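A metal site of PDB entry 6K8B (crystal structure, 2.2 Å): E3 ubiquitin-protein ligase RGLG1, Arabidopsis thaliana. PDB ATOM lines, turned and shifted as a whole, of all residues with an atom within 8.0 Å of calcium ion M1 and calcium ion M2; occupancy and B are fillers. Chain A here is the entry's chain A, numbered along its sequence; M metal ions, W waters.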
ATOM      1  N   SER A  13      20.970   1.565   5.115  1.00  0.00           N
ATOM      2  CA  SER A  13      20.612   2.768   5.870  1.00  0.00           C
ATOM      3  C   SER A  13      19.139   2.741   6.326  1.00  0.00           C
ATOM      4  O   SER A  13      18.355   1.928   5.848  1.00  0.00           O
ATOM      5  CB  SER A  13      20.877   4.026   5.027  1.00  0.00           C
ATOM      6  OG  SER A  13      20.559   5.203   5.749  1.00  0.00           O
ATOM      7  N   LYS A  14      18.775   3.634   7.236  1.00  0.00           N
ATOM      8  CA  LYS A  14      17.425   3.619   7.812  1.00  0.00           C
ATOM      9  C   LYS A  14      16.378   4.190   6.842  1.00  0.00           C
ATOM     10  O   LYS A  14      16.615   5.217   6.209  1.00  0.00           O
ATOM     11  CB  LYS A  14      17.424   4.414   9.133  1.00  0.00           C
ATOM     12  CG  LYS A  14      16.053   4.597   9.759  1.00  0.00           C
ATOM     13  CD  LYS A  14      15.877   6.051  10.215  1.00  0.00           C
ATOM     14  CE  LYS A  14      14.433   6.366  10.567  1.00  0.00           C
ATOM     15  NZ  LYS A  14      14.219   7.819  10.851  1.00  0.00           N
ATOM     16  N   ILE A  15      15.236   3.521   6.723  1.00  0.00           N
ATOM     17  CA  ILE A  15      14.191   3.952   5.787  1.00  0.00           C
ATOM     18  C   ILE A  15      13.110   4.776   6.503  1.00  0.00           C
ATOM     19  O   ILE A  15      12.448   4.306   7.426  1.00  0.00           O
ATOM     20  CB  ILE A  15      13.534   2.745   5.070  1.00  0.00           C
ATOM     21  CG1 ILE A  15      14.538   2.048   4.167  1.00  0.00           C
ATOM     22  CG2 ILE A  15      12.342   3.190   4.242  1.00  0.00           C
ATOM     23  CD1 ILE A  15      14.051   0.703   3.637  1.00  0.00           C
ATOM     24  N   SER A  16      12.923   6.022   6.078  1.00  0.00           N
ATOM     25  CA  SER A  16      11.938   6.884   6.733  1.00  0.00           C
ATOM     26  C   SER A  16      10.560   6.717   6.100  1.00  0.00           C
ATOM     27  O   SER A  16      10.386   5.951   5.149  1.00  0.00           O
ATOM     28  CB  SER A  16      12.389   8.343   6.675  1.00  0.00           C
ATOM     29  OG  SER A  16      13.673   8.491   7.257  1.00  0.00           O
ATOM     30  N   ASP A  17       9.590   7.447   6.637  1.00  0.00           N
ATOM     31  CA  ASP A  17       8.229   7.476   6.093  1.00  0.00           C
ATOM     32  C   ASP A  17       8.156   8.445   4.908  1.00  0.00           C
ATOM     33  O   ASP A  17       7.907   9.627   5.084  1.00  0.00           O
ATOM     34  CB  ASP A  17       7.226   7.868   7.187  1.00  0.00           C
ATOM     35  CG  ASP A  17       7.008   6.741   8.220  1.00  0.00           C
ATOM     36  OD1 ASP A  17       7.732   5.746   8.154  1.00  0.00           O
ATOM     37  OD2 ASP A  17       6.118   6.855   9.085  1.00  0.00           O
ATOM     38  N   ILE A 203      10.226  -7.602   6.422  1.00  0.00           N
ATOM     39  CA  ILE A 203       9.514  -7.963   7.638  1.00  0.00           C
ATOM     40  C   ILE A 203       8.600  -6.817   8.073  1.00  0.00           C
ATOM     41  O   ILE A 203       9.020  -5.649   8.100  1.00  0.00           O
ATOM     42  CB  ILE A 203      10.476  -8.322   8.781  1.00  0.00           C
ATOM     43  CG1 ILE A 203      11.465  -9.393   8.315  1.00  0.00           C
ATOM     44  CG2 ILE A 203       9.692  -8.788  10.003  1.00  0.00           C
ATOM     45  CD1 ILE A 203      12.687  -9.544   9.224  1.00  0.00           C
ATOM     46  N   MET A 216      10.247  -2.717  19.531  1.00  0.00           N
ATOM     47  CA  MET A 216       9.806  -2.861  18.145  1.00  0.00           C
ATOM     48  C   MET A 216      10.281  -1.677  17.297  1.00  0.00           C
ATOM     49  O   MET A 216      10.731  -1.843  16.163  1.00  0.00           O
ATOM     50  CB  MET A 216       8.281  -2.989  18.060  1.00  0.00           C
ATOM     51  CG  MET A 216       7.717  -4.195  18.815  1.00  0.00           C
ATOM     52  SD  MET A 216       8.440  -5.802  18.352  1.00  0.00           S
ATOM     53  CE  MET A 216       9.738  -5.996  19.579  1.00  0.00           C
ATOM     54  N   GLN A 217      10.220  -0.472  17.876  1.00  0.00           N
ATOM     55  CA  GLN A 217      10.699   0.715  17.185  1.00  0.00           C
ATOM     56  C   GLN A 217      12.210   0.671  16.957  1.00  0.00           C
ATOM     57  O   GLN A 217      12.703   1.194  15.961  1.00  0.00           O
ATOM     58  CB  GLN A 217      10.299   1.968  17.969  1.00  0.00           C
ATOM     59  CG  GLN A 217       8.817   2.289  17.826  1.00  0.00           C
ATOM     60  CD  GLN A 217       8.266   3.187  18.938  1.00  0.00           C
ATOM     61  OE1 GLN A 217       8.933   3.444  19.944  1.00  0.00           O
ATOM     62  NE2 GLN A 217       7.034   3.666  18.752  1.00  0.00           N
ATOM     63  N   GLU A 218      12.933   0.036  17.878  1.00  0.00           N
ATOM     64  CA  GLU A 218      14.374  -0.179  17.699  1.00  0.00           C
ATOM     65  C   GLU A 218      14.670  -1.146  16.559  1.00  0.00           C
ATOM     66  O   GLU A 218      15.598  -0.930  15.795  1.00  0.00           O
ATOM     67  CB  GLU A 218      15.017  -0.702  18.988  1.00  0.00           C
ATOM     68  CG  GLU A 218      14.999   0.277  20.163  1.00  0.00           C
ATOM     69  CD  GLU A 218      15.821   1.533  19.916  1.00  0.00           C
ATOM     70  OE1 GLU A 218      16.838   1.460  19.180  1.00  0.00           O
ATOM     71  OE2 GLU A 218      15.436   2.599  20.436  1.00  0.00           O
ATOM     72  N   PHE A 219      13.892  -2.231  16.479  1.00  0.00           N
ATOM     73  CA  PHE A 219      14.004  -3.161  15.372  1.00  0.00           C
ATOM     74  C   PHE A 219      13.728  -2.439  14.053  1.00  0.00           C
ATOM     75  O   PHE A 219      14.396  -2.678  13.029  1.00  0.00           O
ATOM     76  CB  PHE A 219      13.029  -4.340  15.527  1.00  0.00           C
ATOM     77  CG  PHE A 219      13.378  -5.278  16.645  1.00  0.00           C
ATOM     78  CD1 PHE A 219      14.612  -5.225  17.263  1.00  0.00           C
ATOM     79  CD2 PHE A 219      12.440  -6.210  17.090  1.00  0.00           C
ATOM     80  CE1 PHE A 219      14.915  -6.108  18.307  1.00  0.00           C
ATOM     81  CE2 PHE A 219      12.743  -7.086  18.122  1.00  0.00           C
ATOM     82  CZ  PHE A 219      13.980  -7.034  18.731  1.00  0.00           C
ATOM     83  N   ASP A 220      12.737  -1.553  14.093  1.00  0.00           N
ATOM     84  CA  ASP A 220      12.346  -0.766  12.945  1.00  0.00           C
ATOM     85  C   ASP A 220      13.476   0.156  12.466  1.00  0.00           C
ATOM     86  O   ASP A 220      13.791   0.188  11.286  1.00  0.00           O
ATOM     87  CB  ASP A 220      11.084   0.048  13.282  1.00  0.00           C
ATOM     88  CG  ASP A 220      10.482   0.753  12.073  1.00  0.00           C
ATOM     89  OD1 ASP A 220      10.961   0.564  10.933  1.00  0.00           O
ATOM     90  OD2 ASP A 220       9.514   1.519  12.263  1.00  0.00           O
ATOM     91  N   ASP A 221      14.092   0.880  13.402  1.00  0.00           N
ATOM     92  CA  ASP A 221      14.911   2.054  13.066  1.00  0.00           C
ATOM     93  C   ASP A 221      16.409   1.937  13.319  1.00  0.00           C
ATOM     94  O   ASP A 221      17.191   2.720  12.781  1.00  0.00           O
ATOM     95  CB  ASP A 221      14.410   3.269  13.854  1.00  0.00           C
ATOM     96  CG  ASP A 221      13.007   3.680  13.468  1.00  0.00           C
ATOM     97  OD1 ASP A 221      12.653   3.524  12.278  1.00  0.00           O
ATOM     98  OD2 ASP A 221      12.256   4.151  14.342  1.00  0.00           O
ATOM     99  N   ASN A 222      16.836   0.985  14.142  1.00  0.00           N
ATOM    100  CA  ASN A 222      18.175   1.051  14.684  1.00  0.00           C
ATOM    101  C   ASN A 222      18.838  -0.326  14.879  1.00  0.00           C
ATOM    102  O   ASN A 222      18.953  -0.817  15.991  1.00  0.00           O
ATOM    103  CB  ASN A 222      18.150   1.815  16.021  1.00  0.00           C
ATOM    104  CG  ASN A 222      19.532   1.981  16.645  1.00  0.00           C
ATOM    105  OD1 ASN A 222      20.553   2.055  15.944  1.00  0.00           O
ATOM    106  ND2 ASN A 222      19.579   2.035  17.976  1.00  0.00           N
ATOM    107  N   ARG A 226      22.827  -4.667  10.077  1.00  0.00           N
ATOM    108  CA  ARG A 226      22.126  -5.284   8.943  1.00  0.00           C
ATOM    109  C   ARG A 226      22.504  -4.582   7.636  1.00  0.00           C
ATOM    110  O   ARG A 226      23.045  -3.492   7.641  1.00  0.00           O
ATOM    111  CB  ARG A 226      20.616  -5.270   9.154  1.00  0.00           C
ATOM    112  CG  ARG A 226      19.982  -3.902   9.239  1.00  0.00           C
ATOM    113  CD  ARG A 226      18.499  -3.996   9.534  1.00  0.00           C
ATOM    114  NE  ARG A 226      17.970  -2.715  10.001  1.00  0.00           N
ATOM    115  CZ  ARG A 226      16.747  -2.540  10.473  1.00  0.00           C
ATOM    116  NH1 ARG A 226      15.899  -3.551  10.527  1.00  0.00           N
ATOM    117  NH2 ARG A 226      16.367  -1.330  10.896  1.00  0.00           N
ATOM    118  N   PHE A 228      20.484  -3.773   4.971  1.00  0.00           N
ATOM    119  CA  PHE A 228      19.509  -2.746   4.609  1.00  0.00           C
ATOM    120  C   PHE A 228      18.402  -2.759   5.649  1.00  0.00           C
ATOM    121  O   PHE A 228      18.281  -3.714   6.413  1.00  0.00           O
ATOM    122  CB  PHE A 228      18.951  -2.961   3.191  1.00  0.00           C
ATOM    123  CG  PHE A 228      18.046  -4.174   3.040  1.00  0.00           C
ATOM    124  CD1 PHE A 228      18.591  -5.452   2.901  1.00  0.00           C
ATOM    125  CD2 PHE A 228      16.658  -4.030   3.021  1.00  0.00           C
ATOM    126  CE1 PHE A 228      17.761  -6.568   2.747  1.00  0.00           C
ATOM    127  CE2 PHE A 228      15.828  -5.131   2.875  1.00  0.00           C
ATOM    128  CZ  PHE A 228      16.382  -6.405   2.740  1.00  0.00           C
ATOM    129  N   ASP A 229      17.623  -1.690   5.702  1.00  0.00           N
ATOM    130  CA  ASP A 229      16.526  -1.634   6.659  1.00  0.00           C
ATOM    131  C   ASP A 229      15.406  -2.558   6.211  1.00  0.00           C
ATOM    132  O   ASP A 229      14.641  -2.219   5.316  1.00  0.00           O
ATOM    133  CB  ASP A 229      16.034  -0.194   6.808  1.00  0.00           C
ATOM    134  CG  ASP A 229      14.923  -0.052   7.824  1.00  0.00           C
ATOM    135  OD1 ASP A 229      14.477  -1.082   8.385  1.00  0.00           O
ATOM    136  OD2 ASP A 229      14.470   1.099   8.034  1.00  0.00           O
ATOM    137  N   ASN A 230      15.289  -3.730   6.865  1.00  0.00           N
ATOM    138  CA  ASN A 230      14.388  -4.789   6.393  1.00  0.00           C
ATOM    139  C   ASN A 230      13.162  -5.015   7.278  1.00  0.00           C
ATOM    140  O   ASN A 230      12.468  -6.029   7.149  1.00  0.00           O
ATOM    141  CB  ASN A 230      15.171  -6.104   6.246  1.00  0.00           C
ATOM    142  CG  ASN A 230      15.785  -6.582   7.571  1.00  0.00           C
ATOM    143  OD1 ASN A 230      15.800  -5.844   8.564  1.00  0.00           O
ATOM    144  ND2 ASN A 230      16.289  -7.824   7.586  1.00  0.00           N
ATOM    145  N   PHE A 231      12.899  -4.069   8.159  1.00  0.00           N
ATOM    146  CA  PHE A 231      11.946  -4.256   9.251  1.00  0.00           C
ATOM    147  C   PHE A 231      11.095  -3.009   9.433  1.00  0.00           C
ATOM    148  O   PHE A 231      11.628  -1.947   9.716  1.00  0.00           O
ATOM    149  CB  PHE A 231      12.699  -4.575  10.560  1.00  0.00           C
ATOM    150  CG  PHE A 231      11.814  -5.096  11.677  1.00  0.00           C
ATOM    151  CD1 PHE A 231      11.002  -4.236  12.410  1.00  0.00           C
ATOM    152  CD2 PHE A 231      11.840  -6.439  12.033  1.00  0.00           C
ATOM    153  CE1 PHE A 231      10.205  -4.696  13.447  1.00  0.00           C
ATOM    154  CE2 PHE A 231      11.036  -6.910  13.079  1.00  0.00           C
ATOM    155  CZ  PHE A 231      10.231  -6.046  13.782  1.00  0.00           C
ATOM    156  N   GLN A 232       9.786  -3.148   9.282  1.00  0.00           N
ATOM    157  CA  GLN A 232       8.829  -2.082   9.564  1.00  0.00           C
ATOM    158  C   GLN A 232       7.934  -2.451  10.753  1.00  0.00           C
ATOM    159  O   GLN A 232       7.493  -3.596  10.880  1.00  0.00           O
ATOM    160  CB  GLN A 232       7.979  -1.786   8.326  1.00  0.00           C
ATOM    161  CG  GLN A 232       6.705  -0.993   8.561  1.00  0.00           C
ATOM    162  CD  GLN A 232       6.948   0.468   8.941  1.00  0.00           C
ATOM    163  OE1 GLN A 232       7.967   0.815   9.528  1.00  0.00           O
ATOM    164  NE2 GLN A 232       5.993   1.343   8.588  1.00  0.00           N
ATOM    165  N   PHE A 233       7.690  -1.475  11.628  1.00  0.00           N
ATOM    166  CA  PHE A 233       6.770  -1.649  12.743  1.00  0.00           C
ATOM    167  C   PHE A 233       5.443  -0.925  12.488  1.00  0.00           C
ATOM    168  O   PHE A 233       5.437   0.282  12.217  1.00  0.00           O
ATOM    169  CB  PHE A 233       7.399  -1.148  14.040  1.00  0.00           C
ATOM    170  CG  PHE A 233       6.406  -0.978  15.160  1.00  0.00           C
ATOM    171  CD1 PHE A 233       5.658  -2.052  15.602  1.00  0.00           C
ATOM    172  CD2 PHE A 233       6.226   0.268  15.756  1.00  0.00           C
ATOM    173  CE1 PHE A 233       4.731  -1.894  16.631  1.00  0.00           C
ATOM    174  CE2 PHE A 233       5.306   0.431  16.789  1.00  0.00           C
ATOM    175  CZ  PHE A 233       4.559  -0.658  17.222  1.00  0.00           C
ATOM    176  N   VAL A 234       4.340  -1.652  12.540  1.00  0.00           N
ATOM    177  CA  VAL A 234       3.008  -1.056  12.457  1.00  0.00           C
ATOM    178  C   VAL A 234       2.294  -1.127  13.817  1.00  0.00           C
ATOM    179  O   VAL A 234       2.061  -2.217  14.340  1.00  0.00           O
ATOM    180  CB  VAL A 234       2.122  -1.751  11.428  1.00  0.00           C
ATOM    181  CG1 VAL A 234       0.736  -1.108  11.413  1.00  0.00           C
ATOM    182  CG2 VAL A 234       2.768  -1.749  10.036  1.00  0.00           C
ATOM    183  N   SER A 256       0.850   2.150   6.336  1.00  0.00           N
ATOM    184  CA  SER A 256       1.876   1.843   7.345  1.00  0.00           C
ATOM    185  C   SER A 256       2.601   0.526   7.051  1.00  0.00           C
ATOM    186  O   SER A 256       3.824   0.460   7.149  1.00  0.00           O
ATOM    187  CB  SER A 256       1.264   1.782   8.750  1.00  0.00           C
ATOM    188  OG  SER A 256       0.525   2.956   9.027  1.00  0.00           O
ATOM    189  N   MET A 259       4.857   0.831   3.873  1.00  0.00           N
ATOM    190  CA  MET A 259       5.652   2.070   3.837  1.00  0.00           C
ATOM    191  C   MET A 259       7.072   1.876   3.335  1.00  0.00           C
ATOM    192  O   MET A 259       7.595   2.705   2.607  1.00  0.00           O
ATOM    193  CB  MET A 259       5.694   2.714   5.234  1.00  0.00           C
ATOM    194  CG  MET A 259       6.404   4.082   5.308  1.00  0.00           C
ATOM    195  SD  MET A 259       5.536   5.427   4.426  1.00  0.00           S
ATOM    196  CE  MET A 259       4.160   5.769   5.546  1.00  0.00           C
ATOM    197  N   GLU A 260       7.701   0.763   3.742  1.00  0.00           N
ATOM    198  CA  GLU A 260       9.097   0.543   3.422  1.00  0.00           C
ATOM    199  C   GLU A 260       9.283  -0.452   2.292  1.00  0.00           C
ATOM    200  O   GLU A 260      10.408  -0.788   1.932  1.00  0.00           O
ATOM    201  CB  GLU A 260       9.858   0.059   4.658  1.00  0.00           C
ATOM    202  CG  GLU A 260       9.743   0.978   5.866  1.00  0.00           C
ATOM    203  CD  GLU A 260      10.673   0.576   7.001  1.00  0.00           C
ATOM    204  OE1 GLU A 260      11.580  -0.247   6.770  1.00  0.00           O
ATOM    205  OE2 GLU A 260      10.497   1.091   8.129  1.00  0.00           O
ATOM    206  N   GLN A 264      12.699  -1.357   0.152  1.00  0.00           N
ATOM    207  CA  GLN A 264      13.246  -2.660   0.539  1.00  0.00           C
ATOM    208  C   GLN A 264      13.352  -3.555  -0.687  1.00  0.00           C
ATOM    209  O   GLN A 264      14.378  -4.198  -0.913  1.00  0.00           O
ATOM    210  CB  GLN A 264      12.397  -3.339   1.630  1.00  0.00           C
ATOM    211  CG  GLN A 264      12.678  -2.754   2.988  1.00  0.00           C
ATOM    212  CD  GLN A 264      11.686  -3.195   4.055  1.00  0.00           C
ATOM    213  OE1 GLN A 264      10.716  -3.893   3.787  1.00  0.00           O
ATOM    214  NE2 GLN A 264      11.933  -2.758   5.288  1.00  0.00           N
HETATM  215 CA    CA M   1       9.636   2.412   9.802  1.00  0.00          CA
HETATM  216 CA    CA M   2      12.508   0.183   9.232  1.00  0.00          CA
HETATM  217  O   HOH W   1       7.512   3.620  10.111  1.00  0.00           O
HETATM  218  O   HOH W   2      10.341   4.175  11.333  1.00  0.00           O
HETATM  219  O   HOH W   3      12.317   2.699   9.700  1.00  0.00           O
HETATM  220  O   HOH W   4       9.758   4.149   7.948  1.00  0.00           O
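Calcium ion M1 is bound by OE2 of Glu 260 (2.3 Å), OE1 of Gln 232 (2.3 Å), water W2 (2.4 Å), water W1 (2.5 Å), OD1 of Asp 220 (2.5 Å), water W4 (2.5 Å), OD2 of Asp 220 (2.6 Å) and water W3 (2.7 Å).
Calcium ion M1 has eight donor atoms within binding distance.
Water W1 bridges the side-chain carboxylate (OD1) of Asp 17 and the side-chain amide nitrogen (NE2) of Gln 232.
Water W3 bridges the side-chain carboxylate (OD1) of Asp 221 (2.7 Å) and the backbone carbonyl oxygen (O) of Ile 15 (2.8 Å).
Four residues have an atom within 4 Å of calcium ion M2: Asp 220, Asp 229, Phe 231 and Glu 260.
The nearest printed residue that does not touch calcium ion M2 is Gln 232 (4.3 Å).
NH2 of Arg 226 sits close to OD1 of Asp 229.
The side-chain carboxylate of Asp 229 lies close to the backbone NH of Ile 15, at 2.9 Å.
The backbone carbonyl oxygen (O) of Ile 203 is in hydrogen-bond range of the backbone NH (N) of Gln 232, 2.9 Å away.
The backbone carbonyl oxygen (O) of Ser 256 lies within hydrogen-bond range of the side-chain amide nitrogen (NE2) of Gln 232 (2.7 Å).
NH2 of Arg 226 lies close to O of Asp 220, at 3.0 Å.
NE2 of Gln 264 lies close to OE1 of Glu 260 (2.9 Å).
The side-chain amide nitrogen (NE2) of Gln 264 sits at hydrogen-bond distance from the backbone carbonyl oxygen (O) of Asp 229, at 2.8 Å.
N of Phe 231 sits close to NE2 of Gln 264 (3.3 Å).
Calcium ion M2 is bound by OD1 of Asp 220, 2.3 Å away.
Calcium ion M2 is bound by the backbone carbonyl oxygen (O) of Phe 231, at 2.4 Å.
O of Asp 220 is bound to calcium ion M2 (2.4 Å).
OE2 of Glu 260 is bound to calcium ion M2 (2.5 Å).
OD2 of Asp 229 is bound to calcium ion M2 (2.5 Å).
The side-chain carboxylate (OD1) of Asp 229 is bound to calcium ion M2 (2.5 Å).
Calcium ion M2 is bound by water W3, at 2.6 Å.
Calcium ion M2 is bound by OE1 of Glu 260 (2.7 Å).
Calcium ion M2 has eight donor atoms within binding distance.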
